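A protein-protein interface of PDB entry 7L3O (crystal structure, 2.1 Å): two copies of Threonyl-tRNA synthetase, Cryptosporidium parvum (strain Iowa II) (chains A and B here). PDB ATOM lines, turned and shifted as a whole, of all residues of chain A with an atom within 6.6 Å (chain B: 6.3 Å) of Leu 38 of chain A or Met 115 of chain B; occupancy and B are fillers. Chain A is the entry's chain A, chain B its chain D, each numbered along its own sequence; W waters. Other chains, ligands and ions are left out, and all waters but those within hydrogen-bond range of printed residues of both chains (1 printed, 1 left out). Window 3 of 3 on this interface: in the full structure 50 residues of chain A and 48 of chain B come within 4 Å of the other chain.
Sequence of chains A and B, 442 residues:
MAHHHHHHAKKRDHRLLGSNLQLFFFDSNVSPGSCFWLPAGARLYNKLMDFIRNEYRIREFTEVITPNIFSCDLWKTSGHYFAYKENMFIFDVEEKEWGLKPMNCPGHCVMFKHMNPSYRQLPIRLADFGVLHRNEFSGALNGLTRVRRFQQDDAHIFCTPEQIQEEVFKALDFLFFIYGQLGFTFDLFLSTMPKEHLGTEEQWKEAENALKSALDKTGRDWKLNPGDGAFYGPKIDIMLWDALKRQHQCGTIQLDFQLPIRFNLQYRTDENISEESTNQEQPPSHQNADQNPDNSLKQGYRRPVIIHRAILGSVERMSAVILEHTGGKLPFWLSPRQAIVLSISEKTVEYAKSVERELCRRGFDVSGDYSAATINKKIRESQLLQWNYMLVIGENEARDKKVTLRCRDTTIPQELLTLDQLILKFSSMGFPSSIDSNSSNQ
The backbone carbonyl oxygen of Ile 65 of chain B is in hydrogen-bond range of the backbone NH of Trp 37 of chain A (2.8 Å).
The backbone NH (N) of Leu 38 of chain A lies within hydrogen-bond range of the backbone carbonyl oxygen (O) of Leu 23 of chain A (2.9 Å). O of Phe 25 of chain A lies within hydrogen-bond range of N of Phe 36 of chain A, at 2.9 Å.
CD1 of Phe 25 of chain A touches CD2 of His 114 of chain B (3.5 Å). O of Ile 65 of chain B touches C of Phe 36 of chain A, 3.7 Å away. CG of Met 111 of chain B touches CD2 of Phe 36 of chain A, at 3.7 Å. Trp 37 of chain A touches Val 64 of chain B. Met 111 of chain B touches Trp 37 of chain A. Pro 39 of chain A touches Glu 63 of chain B. Val 64 of chain B touches Pro 39 of chain A (CG1 to CD, 3.8 Å). O of Glu 63 of chain B touches CB of Ala 42 of chain A, at 3.5 Å. Val 64 of chain B touches Ala 42 of chain A (CA to CB, 3.98 Å). Ala 42 of chain A touches Ile 65 of chain B (CB to CG1, 3.9 Å).
Of the printed residues of chain B, Phe 25 of chain A touches His 114. Leu 38 of chain A touches just these residues of chain B: Met 111 and Met 115. Of the printed residues of chain B, Ala 42 of chain A touches Glu 63, Val 64 and Ile 65. Printed residues of chain A within 4 Å of Thr 62 of chain B: Pro 39 (3.5 Å). Printed residues of chain A within 4 Å of Glu 63 of chain B: Pro 39 (3.6 Å) and Ala 42 (3.5 Å). Phe 112 of chain B touches none of the printed residues of chain A. Of the printed residues of chain A, His 114 of chain B touches Phe 25. Ser 118 of chain B touches none of the printed residues of chain A. The nearest residue of chain B that does not touch Leu 38 of chain A is His 114 of chain B (4.2 Å). The nearest residue of chain A that does not touch Met 115 of chain B is Pro 39 of chain A (4.7 Å). The nearest printed residue of chain B that does not touch Trp 37 of chain A is Glu 63 of chain B (5.1 Å).
Hydrophobic or aromatic side chains of chain B within 4 Å of the printed part of chain A: Val 64, Ile 65, Met 111, His 114 and Met 115. Hydrophobic or aromatic side chains of chain A that line the printed part of chain B: Phe 25, Phe 36, Trp 37, Leu 38, Pro 39 and Ala 42. Among the printed residues, no Asp or Glu carboxylate lies within 4 Å of a Lys or Arg side-chain nitrogen of the other chain.
No position is printed for both chains. Of the 14 pairs that touch across the chains among the printed residues, none has its exchanged pair printed and touching as well.
Water W1 bridges O of Glu 63 of chain B and O of Pro 39 of chain A.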
ATOM      1  N   GLY A  18      15.787  18.818   0.011  1.00  0.00           N
ATOM      2  CA  GLY A  18      15.559  18.860   1.448  1.00  0.00           C
ATOM      3  C   GLY A  18      16.348  17.824   2.214  1.00  0.00           C
ATOM      4  O   GLY A  18      16.646  18.030   3.397  1.00  0.00           O
ATOM      5  N   SER A  19      16.709  16.724   1.563  1.00  0.00           N
ATOM      6  CA  SER A  19      17.536  15.729   2.225  1.00  0.00           C
ATOM      7  C   SER A  19      19.012  16.094   2.130  1.00  0.00           C
ATOM      8  O   SER A  19      19.741  16.016   3.124  1.00  0.00           O
ATOM      9  CB  SER A  19      17.278  14.346   1.624  1.00  0.00           C
ATOM     10  OG  SER A  19      18.318  13.451   1.981  1.00  0.00           O
ATOM     11  N   LEU A  21      20.359  19.027   1.657  1.00  0.00           N
ATOM     12  CA  LEU A  21      20.626  20.239   2.409  1.00  0.00           C
ATOM     13  C   LEU A  21      20.164  20.146   3.850  1.00  0.00           C
ATOM     14  O   LEU A  21      20.168  21.162   4.542  1.00  0.00           O
ATOM     15  CB  LEU A  21      19.971  21.434   1.723  1.00  0.00           C
ATOM     16  CG  LEU A  21      20.467  21.586   0.290  1.00  0.00           C
ATOM     17  CD1 LEU A  21      19.742  22.709  -0.431  1.00  0.00           C
ATOM     18  CD2 LEU A  21      21.974  21.807   0.294  1.00  0.00           C
ATOM     19  N   GLN A  22      19.769  18.959   4.311  1.00  0.00           N
ATOM     20  CA  GLN A  22      19.337  18.745   5.692  1.00  0.00           C
ATOM     21  C   GLN A  22      18.302  19.786   6.112  1.00  0.00           C
ATOM     22  O   GLN A  22      18.414  20.432   7.154  1.00  0.00           O
ATOM     23  CB  GLN A  22      20.539  18.735   6.643  1.00  0.00           C
ATOM     24  CG  GLN A  22      21.597  17.696   6.251  1.00  0.00           C
ATOM     25  CD  GLN A  22      22.812  17.758   7.160  1.00  0.00           C
ATOM     26  OE1 GLN A  22      22.684  17.922   8.374  1.00  0.00           O
ATOM     27  NE2 GLN A  22      23.985  17.659   6.579  1.00  0.00           N
ATOM     28  N   LEU A  23      17.291  19.958   5.265  1.00  0.00           N
ATOM     29  CA  LEU A  23      16.228  20.915   5.514  1.00  0.00           C
ATOM     30  C   LEU A  23      15.016  20.259   6.161  1.00  0.00           C
ATOM     31  O   LEU A  23      14.475  20.792   7.127  1.00  0.00           O
ATOM     32  CB  LEU A  23      15.797  21.584   4.209  1.00  0.00           C
ATOM     33  CG  LEU A  23      16.836  22.417   3.477  1.00  0.00           C
ATOM     34  CD1 LEU A  23      16.167  23.102   2.270  1.00  0.00           C
ATOM     35  CD2 LEU A  23      17.429  23.422   4.435  1.00  0.00           C
ATOM     36  N   PHE A  24      14.567  19.122   5.626  1.00  0.00           N
ATOM     37  CA  PHE A  24      13.351  18.467   6.094  1.00  0.00           C
ATOM     38  C   PHE A  24      13.328  17.024   5.600  1.00  0.00           C
ATOM     39  O   PHE A  24      14.050  16.656   4.677  1.00  0.00           O
ATOM     40  CB  PHE A  24      12.098  19.208   5.608  1.00  0.00           C
ATOM     41  CG  PHE A  24      12.109  19.507   4.129  1.00  0.00           C
ATOM     42  CD1 PHE A  24      11.819  18.512   3.196  1.00  0.00           C
ATOM     43  CD2 PHE A  24      12.406  20.783   3.670  1.00  0.00           C
ATOM     44  CE1 PHE A  24      11.823  18.792   1.830  1.00  0.00           C
ATOM     45  CE2 PHE A  24      12.416  21.073   2.307  1.00  0.00           C
ATOM     46  CZ  PHE A  24      12.130  20.068   1.383  1.00  0.00           C
ATOM     47  N   PHE A  25      12.474  16.220   6.227  1.00  0.00           N
ATOM     48  CA  PHE A  25      12.274  14.846   5.807  1.00  0.00           C
ATOM     49  C   PHE A  25      10.848  14.443   6.140  1.00  0.00           C
ATOM     50  O   PHE A  25      10.130  15.142   6.859  1.00  0.00           O
ATOM     51  CB  PHE A  25      13.270  13.895   6.470  1.00  0.00           C
ATOM     52  CG  PHE A  25      13.053  13.726   7.944  1.00  0.00           C
ATOM     53  CD1 PHE A  25      13.635  14.599   8.843  1.00  0.00           C
ATOM     54  CD2 PHE A  25      12.272  12.691   8.435  1.00  0.00           C
ATOM     55  CE1 PHE A  25      13.445  14.444  10.205  1.00  0.00           C
ATOM     56  CE2 PHE A  25      12.077  12.534   9.793  1.00  0.00           C
ATOM     57  CZ  PHE A  25      12.663  13.414  10.683  1.00  0.00           C
ATOM     58  N   PHE A  36       8.627  16.821   8.665  1.00  0.00           N
ATOM     59  CA  PHE A  36       9.551  17.104   9.757  1.00  0.00           C
ATOM     60  C   PHE A  36      10.572  18.118   9.252  1.00  0.00           C
ATOM     61  O   PHE A  36      11.412  17.787   8.415  1.00  0.00           O
ATOM     62  CB  PHE A  36      10.246  15.830  10.235  1.00  0.00           C
ATOM     63  CG  PHE A  36       9.348  14.866  10.984  1.00  0.00           C
ATOM     64  CD1 PHE A  36       8.478  14.031  10.303  1.00  0.00           C
ATOM     65  CD2 PHE A  36       9.399  14.777  12.370  1.00  0.00           C
ATOM     66  CE1 PHE A  36       7.662  13.132  10.985  1.00  0.00           C
ATOM     67  CE2 PHE A  36       8.584  13.873  13.061  1.00  0.00           C
ATOM     68  CZ  PHE A  36       7.721  13.046  12.355  1.00  0.00           C
ATOM     69  N   TRP A  37      10.507  19.350   9.755  1.00  0.00           N
ATOM     70  CA  TRP A  37      11.467  20.371   9.355  1.00  0.00           C
ATOM     71  C   TRP A  37      12.635  20.368  10.340  1.00  0.00           C
ATOM     72  O   TRP A  37      12.457  20.634  11.531  1.00  0.00           O
ATOM     73  CB  TRP A  37      10.805  21.748   9.281  1.00  0.00           C
ATOM     74  CG  TRP A  37       9.715  21.823   8.263  1.00  0.00           C
ATOM     75  CD1 TRP A  37       8.458  21.313   8.373  1.00  0.00           C
ATOM     76  CD2 TRP A  37       9.791  22.431   6.969  1.00  0.00           C
ATOM     77  NE1 TRP A  37       7.740  21.569   7.229  1.00  0.00           N
ATOM     78  CE2 TRP A  37       8.537  22.254   6.351  1.00  0.00           C
ATOM     79  CE3 TRP A  37      10.799  23.101   6.270  1.00  0.00           C
ATOM     80  CZ2 TRP A  37       8.262  22.730   5.069  1.00  0.00           C
ATOM     81  CZ3 TRP A  37      10.524  23.575   5.000  1.00  0.00           C
ATOM     82  CH2 TRP A  37       9.268  23.382   4.409  1.00  0.00           C
ATOM     83  N   LEU A  38      13.816  20.025   9.839  1.00  0.00           N
ATOM     84  CA  LEU A  38      15.057  20.081  10.590  1.00  0.00           C
ATOM     85  C   LEU A  38      15.399  21.539  10.869  1.00  0.00           C
ATOM     86  O   LEU A  38      14.807  22.437  10.269  1.00  0.00           O
ATOM     87  CB  LEU A  38      16.161  19.392   9.787  1.00  0.00           C
ATOM     88  CG  LEU A  38      16.023  17.883   9.604  1.00  0.00           C
ATOM     89  CD1 LEU A  38      16.859  17.424   8.415  1.00  0.00           C
ATOM     90  CD2 LEU A  38      16.480  17.164  10.865  1.00  0.00           C
ATOM     91  N   PRO A  39      16.361  21.815  11.781  1.00  0.00           N
ATOM     92  CA  PRO A  39      16.683  23.214  12.124  1.00  0.00           C
ATOM     93  C   PRO A  39      16.814  24.161  10.937  1.00  0.00           C
ATOM     94  O   PRO A  39      16.197  25.230  10.934  1.00  0.00           O
ATOM     95  CB  PRO A  39      18.015  23.080  12.866  1.00  0.00           C
ATOM     96  CG  PRO A  39      17.875  21.785  13.589  1.00  0.00           C
ATOM     97  CD  PRO A  39      17.126  20.869  12.626  1.00  0.00           C
ATOM     98  N   ALA A  40      17.597  23.781   9.920  1.00  0.00           N
ATOM     99  CA  ALA A  40      17.819  24.682   8.794  1.00  0.00           C
ATOM    100  C   ALA A  40      16.544  24.868   7.977  1.00  0.00           C
ATOM    101  O   ALA A  40      16.299  25.955   7.442  1.00  0.00           O
ATOM    102  CB  ALA A  40      18.950  24.163   7.908  1.00  0.00           C
ATOM    103  N   GLY A  41      15.726  23.818   7.860  1.00  0.00           N
ATOM    104  CA  GLY A  41      14.474  23.952   7.128  1.00  0.00           C
ATOM    105  C   GLY A  41      13.502  24.870   7.843  1.00  0.00           C
ATOM    106  O   GLY A  41      12.861  25.722   7.222  1.00  0.00           O
ATOM    107  N   ALA A  42      13.396  24.724   9.171  1.00  0.00           N
ATOM    108  CA  ALA A  42      12.538  25.613   9.937  1.00  0.00           C
ATOM    109  C   ALA A  42      12.996  27.061   9.831  1.00  0.00           C
ATOM    110  O   ALA A  42      12.158  27.970   9.836  1.00  0.00           O
ATOM    111  CB  ALA A  42      12.480  25.168  11.396  1.00  0.00           C
ATOM    112  N   ARG A  43      14.313  27.304   9.740  1.00  0.00           N
ATOM    113  CA  ARG A  43      14.778  28.676   9.526  1.00  0.00           C
ATOM    114  C   ARG A  43      14.230  29.236   8.210  1.00  0.00           C
ATOM    115  O   ARG A  43      13.748  30.371   8.156  1.00  0.00           O
ATOM    116  CB  ARG A  43      16.312  28.739   9.560  1.00  0.00           C
ATOM    117  CG  ARG A  43      16.915  28.351  10.933  1.00  0.00           C
ATOM    118  CD  ARG A  43      18.321  28.896  11.172  1.00  0.00           C
ATOM    119  NE  ARG A  43      19.319  28.243  10.329  1.00  0.00           N
ATOM    120  CZ  ARG A  43      19.911  27.098  10.633  1.00  0.00           C
ATOM    121  NH1 ARG A  43      19.619  26.448  11.749  1.00  0.00           N
ATOM    122  NH2 ARG A  43      20.821  26.593   9.799  1.00  0.00           N
ATOM    123  N   THR B  62      17.888  25.099  18.613  1.00  0.00           N
ATOM    124  CA  THR B  62      17.455  25.125  17.217  1.00  0.00           C
ATOM    125  C   THR B  62      15.985  24.760  17.154  1.00  0.00           C
ATOM    126  O   THR B  62      15.604  23.629  17.486  1.00  0.00           O
ATOM    127  CB  THR B  62      18.280  24.180  16.343  1.00  0.00           C
ATOM    128  OG1 THR B  62      18.230  22.866  16.898  1.00  0.00           O
ATOM    129  CG2 THR B  62      19.739  24.635  16.286  1.00  0.00           C
ATOM    130  N   GLU B  63      15.169  25.721  16.740  1.00  0.00           N
ATOM    131  CA  GLU B  63      13.755  25.471  16.534  1.00  0.00           C
ATOM    132  C   GLU B  63      13.539  24.481  15.393  1.00  0.00           C
ATOM    133  O   GLU B  63      14.232  24.508  14.365  1.00  0.00           O
ATOM    134  CB  GLU B  63      13.029  26.782  16.239  1.00  0.00           C
ATOM    135  CG  GLU B  63      11.506  26.645  16.228  1.00  0.00           C
ATOM    136  CD  GLU B  63      10.761  27.977  16.160  1.00  0.00           C
ATOM    137  OE1 GLU B  63      11.386  29.058  16.261  1.00  0.00           O
ATOM    138  OE2 GLU B  63       9.532  27.934  16.017  1.00  0.00           O
ATOM    139  N   VAL B  64      12.567  23.594  15.573  1.00  0.00           N
ATOM    140  CA  VAL B  64      12.149  22.707  14.501  1.00  0.00           C
ATOM    141  C   VAL B  64      10.639  22.820  14.353  1.00  0.00           C
ATOM    142  O   VAL B  64       9.958  23.457  15.156  1.00  0.00           O
ATOM    143  CB  VAL B  64      12.578  21.247  14.738  1.00  0.00           C
ATOM    144  CG1 VAL B  64      14.071  21.167  14.924  1.00  0.00           C
ATOM    145  CG2 VAL B  64      11.849  20.664  15.922  1.00  0.00           C
ATOM    146  N   ILE B  65      10.125  22.230  13.280  1.00  0.00           N
ATOM    147  CA  ILE B  65       8.693  22.164  13.027  1.00  0.00           C
ATOM    148  C   ILE B  65       8.333  20.708  12.796  1.00  0.00           C
ATOM    149  O   ILE B  65       8.954  20.038  11.966  1.00  0.00           O
ATOM    150  CB  ILE B  65       8.279  23.031  11.821  1.00  0.00           C
ATOM    151  CG1 ILE B  65       8.683  24.487  12.058  1.00  0.00           C
ATOM    152  CG2 ILE B  65       6.772  22.928  11.589  1.00  0.00           C
ATOM    153  CD1 ILE B  65       8.573  25.340  10.820  1.00  0.00           C
ATOM    154  N   VAL B 110      11.875  10.971  16.972  1.00  0.00           N
ATOM    155  CA  VAL B 110      11.970  10.574  15.572  1.00  0.00           C
ATOM    156  C   VAL B 110      13.012  11.420  14.855  1.00  0.00           C
ATOM    157  O   VAL B 110      13.804  10.908  14.055  1.00  0.00           O
ATOM    158  CB  VAL B 110      10.589  10.664  14.895  1.00  0.00           C
ATOM    159  CG1 VAL B 110      10.720  10.429  13.391  1.00  0.00           C
ATOM    160  CG2 VAL B 110       9.643   9.624  15.507  1.00  0.00           C
ATOM    161  N   MET B 111      13.053  12.722  15.161  1.00  0.00           N
ATOM    162  CA  MET B 111      14.026  13.606  14.526  1.00  0.00           C
ATOM    163  C   MET B 111      15.440  13.261  14.953  1.00  0.00           C
ATOM    164  O   MET B 111      16.346  13.181  14.118  1.00  0.00           O
ATOM    165  CB  MET B 111      13.719  15.068  14.857  1.00  0.00           C
ATOM    166  CG  MET B 111      12.542  15.597  14.095  1.00  0.00           C
ATOM    167  SD  MET B 111      12.483  17.382  14.016  1.00  0.00           S
ATOM    168  CE  MET B 111      14.172  17.784  13.611  1.00  0.00           C
ATOM    169  N   PHE B 112      15.653  13.081  16.255  1.00  0.00           N
ATOM    170  CA  PHE B 112      16.959  12.646  16.730  1.00  0.00           C
ATOM    171  C   PHE B 112      17.404  11.394  16.002  1.00  0.00           C
ATOM    172  O   PHE B 112      18.546  11.303  15.537  1.00  0.00           O
ATOM    173  CB  PHE B 112      16.928  12.393  18.238  1.00  0.00           C
ATOM    174  CG  PHE B 112      18.263  12.034  18.809  1.00  0.00           C
ATOM    175  CD1 PHE B 112      19.121  13.019  19.267  1.00  0.00           C
ATOM    176  CD2 PHE B 112      18.665  10.713  18.887  1.00  0.00           C
ATOM    177  CE1 PHE B 112      20.350  12.697  19.790  1.00  0.00           C
ATOM    178  CE2 PHE B 112      19.902  10.379  19.406  1.00  0.00           C
ATOM    179  CZ  PHE B 112      20.745  11.372  19.860  1.00  0.00           C
ATOM    180  N   LYS B 113      16.507  10.410  15.895  1.00  0.00           N
ATOM    181  CA  LYS B 113      16.831   9.196  15.154  1.00  0.00           C
ATOM    182  C   LYS B 113      17.284   9.532  13.742  1.00  0.00           C
ATOM    183  O   LYS B 113      18.335   9.070  13.286  1.00  0.00           O
ATOM    184  CB  LYS B 113      15.624   8.259  15.117  1.00  0.00           C
ATOM    185  CG  LYS B 113      15.529   7.342  16.305  1.00  0.00           C
ATOM    186  CD  LYS B 113      14.364   6.384  16.190  1.00  0.00           C
ATOM    187  CE  LYS B 113      14.754   5.158  15.402  1.00  0.00           C
ATOM    188  NZ  LYS B 113      15.761   4.352  16.148  1.00  0.00           N
ATOM    189  N   HIS B 114      16.510  10.365  13.045  1.00  0.00           N
ATOM    190  CA  HIS B 114      16.873  10.743  11.688  1.00  0.00           C
ATOM    191  C   HIS B 114      18.229  11.431  11.653  1.00  0.00           C
ATOM    192  O   HIS B 114      19.076  11.104  10.820  1.00  0.00           O
ATOM    193  CB  HIS B 114      15.811  11.659  11.084  1.00  0.00           C
ATOM    194  CG  HIS B 114      16.175  12.157   9.719  1.00  0.00           C
ATOM    195  ND1 HIS B 114      15.928  11.434   8.573  1.00  0.00           N
ATOM    196  CD2 HIS B 114      16.812  13.284   9.325  1.00  0.00           C
ATOM    197  CE1 HIS B 114      16.373  12.109   7.528  1.00  0.00           C
ATOM    198  NE2 HIS B 114      16.913  13.236   7.957  1.00  0.00           N
ATOM    199  N   MET B 115      18.447  12.401  12.546  1.00  0.00           N
ATOM    200  CA  MET B 115      19.697  13.154  12.521  1.00  0.00           C
ATOM    201  C   MET B 115      20.902  12.254  12.770  1.00  0.00           C
ATOM    202  O   MET B 115      21.994  12.535  12.264  1.00  0.00           O
ATOM    203  CB  MET B 115      19.654  14.291  13.550  1.00  0.00           C
ATOM    204  CG  MET B 115      18.527  15.285  13.331  1.00  0.00           C
ATOM    205  SD  MET B 115      18.292  16.444  14.719  1.00  0.00           S
ATOM    206  CE  MET B 115      19.752  17.480  14.510  1.00  0.00           C
ATOM    207  N   ASN B 116      20.731  11.182  13.540  1.00  0.00           N
ATOM    208  CA  ASN B 116      21.768  10.174  13.732  1.00  0.00           C
ATOM    209  C   ASN B 116      23.130  10.778  14.086  1.00  0.00           C
ATOM    210  O   ASN B 116      24.119  10.553  13.376  1.00  0.00           O
ATOM    211  CB  ASN B 116      21.875   9.308  12.485  1.00  0.00           C
ATOM    212  CG  ASN B 116      22.686   8.058  12.711  1.00  0.00           C
ATOM    213  OD1 ASN B 116      22.586   7.423  13.759  1.00  0.00           O
ATOM    214  ND2 ASN B 116      23.500   7.694  11.723  1.00  0.00           N
ATOM    215  N   PRO B 117      23.222  11.552  15.159  1.00  0.00           N
ATOM    216  CA  PRO B 117      24.461  12.280  15.436  1.00  0.00           C
ATOM    217  C   PRO B 117      25.488  11.405  16.142  1.00  0.00           C
ATOM    218  O   PRO B 117      25.174  10.350  16.694  1.00  0.00           O
ATOM    219  CB  PRO B 117      23.990  13.412  16.350  1.00  0.00           C
ATOM    220  CG  PRO B 117      22.907  12.768  17.136  1.00  0.00           C
ATOM    221  CD  PRO B 117      22.206  11.808  16.193  1.00  0.00           C
ATOM    222  N   SER B 118      26.738  11.866  16.099  1.00  0.00           N
ATOM    223  CA  SER B 118      27.800  11.343  16.946  1.00  0.00           C
ATOM    224  C   SER B 118      27.949  12.233  18.177  1.00  0.00           C
ATOM    225  O   SER B 118      27.262  13.248  18.329  1.00  0.00           O
ATOM    226  CB  SER B 118      29.126  11.276  16.195  1.00  0.00           C
ATOM    227  OG  SER B 118      29.698  12.570  16.116  1.00  0.00           O
ATOM    228  N   GLN B 121      28.589  16.100  18.012  1.00  0.00           N
ATOM    229  CA  GLN B 121      27.491  17.016  17.754  1.00  0.00           C
ATOM    230  C   GLN B 121      26.497  17.112  18.909  1.00  0.00           C
ATOM    231  O   GLN B 121      25.531  17.877  18.817  1.00  0.00           O
ATOM    232  CB  GLN B 121      26.802  16.602  16.455  1.00  0.00           C
ATOM    233  CG  GLN B 121      27.806  16.620  15.292  1.00  0.00           C
ATOM    234  CD  GLN B 121      27.355  15.838  14.079  1.00  0.00           C
ATOM    235  OE1 GLN B 121      26.629  14.850  14.195  1.00  0.00           O
ATOM    236  NE2 GLN B 121      27.788  16.277  12.900  1.00  0.00           N
ATOM    237  N   ILE B 124      22.257  18.133  21.394  1.00  0.00           N
ATOM    238  CA  ILE B 124      21.257  18.593  20.441  1.00  0.00           C
ATOM    239  C   ILE B 124      20.087  19.145  21.238  1.00  0.00           C
ATOM    240  O   ILE B 124      19.654  18.534  22.226  1.00  0.00           O
ATOM    241  CB  ILE B 124      20.811  17.453  19.509  1.00  0.00           C
ATOM    242  CG1 ILE B 124      21.941  17.093  18.555  1.00  0.00           C
ATOM    243  CG2 ILE B 124      19.549  17.836  18.747  1.00  0.00           C
ATOM    244  CD1 ILE B 124      21.609  15.931  17.686  1.00  0.00           C
ATOM    245  N   LEU B 126      16.409  20.610  20.507  1.00  0.00           N
ATOM    246  CA  LEU B 126      15.323  20.830  19.559  1.00  0.00           C
ATOM    247  C   LEU B 126      14.204  21.577  20.263  1.00  0.00           C
ATOM    248  O   LEU B 126      13.639  21.074  21.241  1.00  0.00           O
ATOM    249  CB  LEU B 126      14.808  19.508  18.981  1.00  0.00           C
ATOM    250  CG  LEU B 126      15.834  18.642  18.259  1.00  0.00           C
ATOM    251  CD1 LEU B 126      15.184  17.413  17.578  1.00  0.00           C
ATOM    252  CD2 LEU B 126      16.593  19.488  17.248  1.00  0.00           C
HETATM  253  O   HOH W   1      15.489  26.411  13.154  1.00  0.00           O
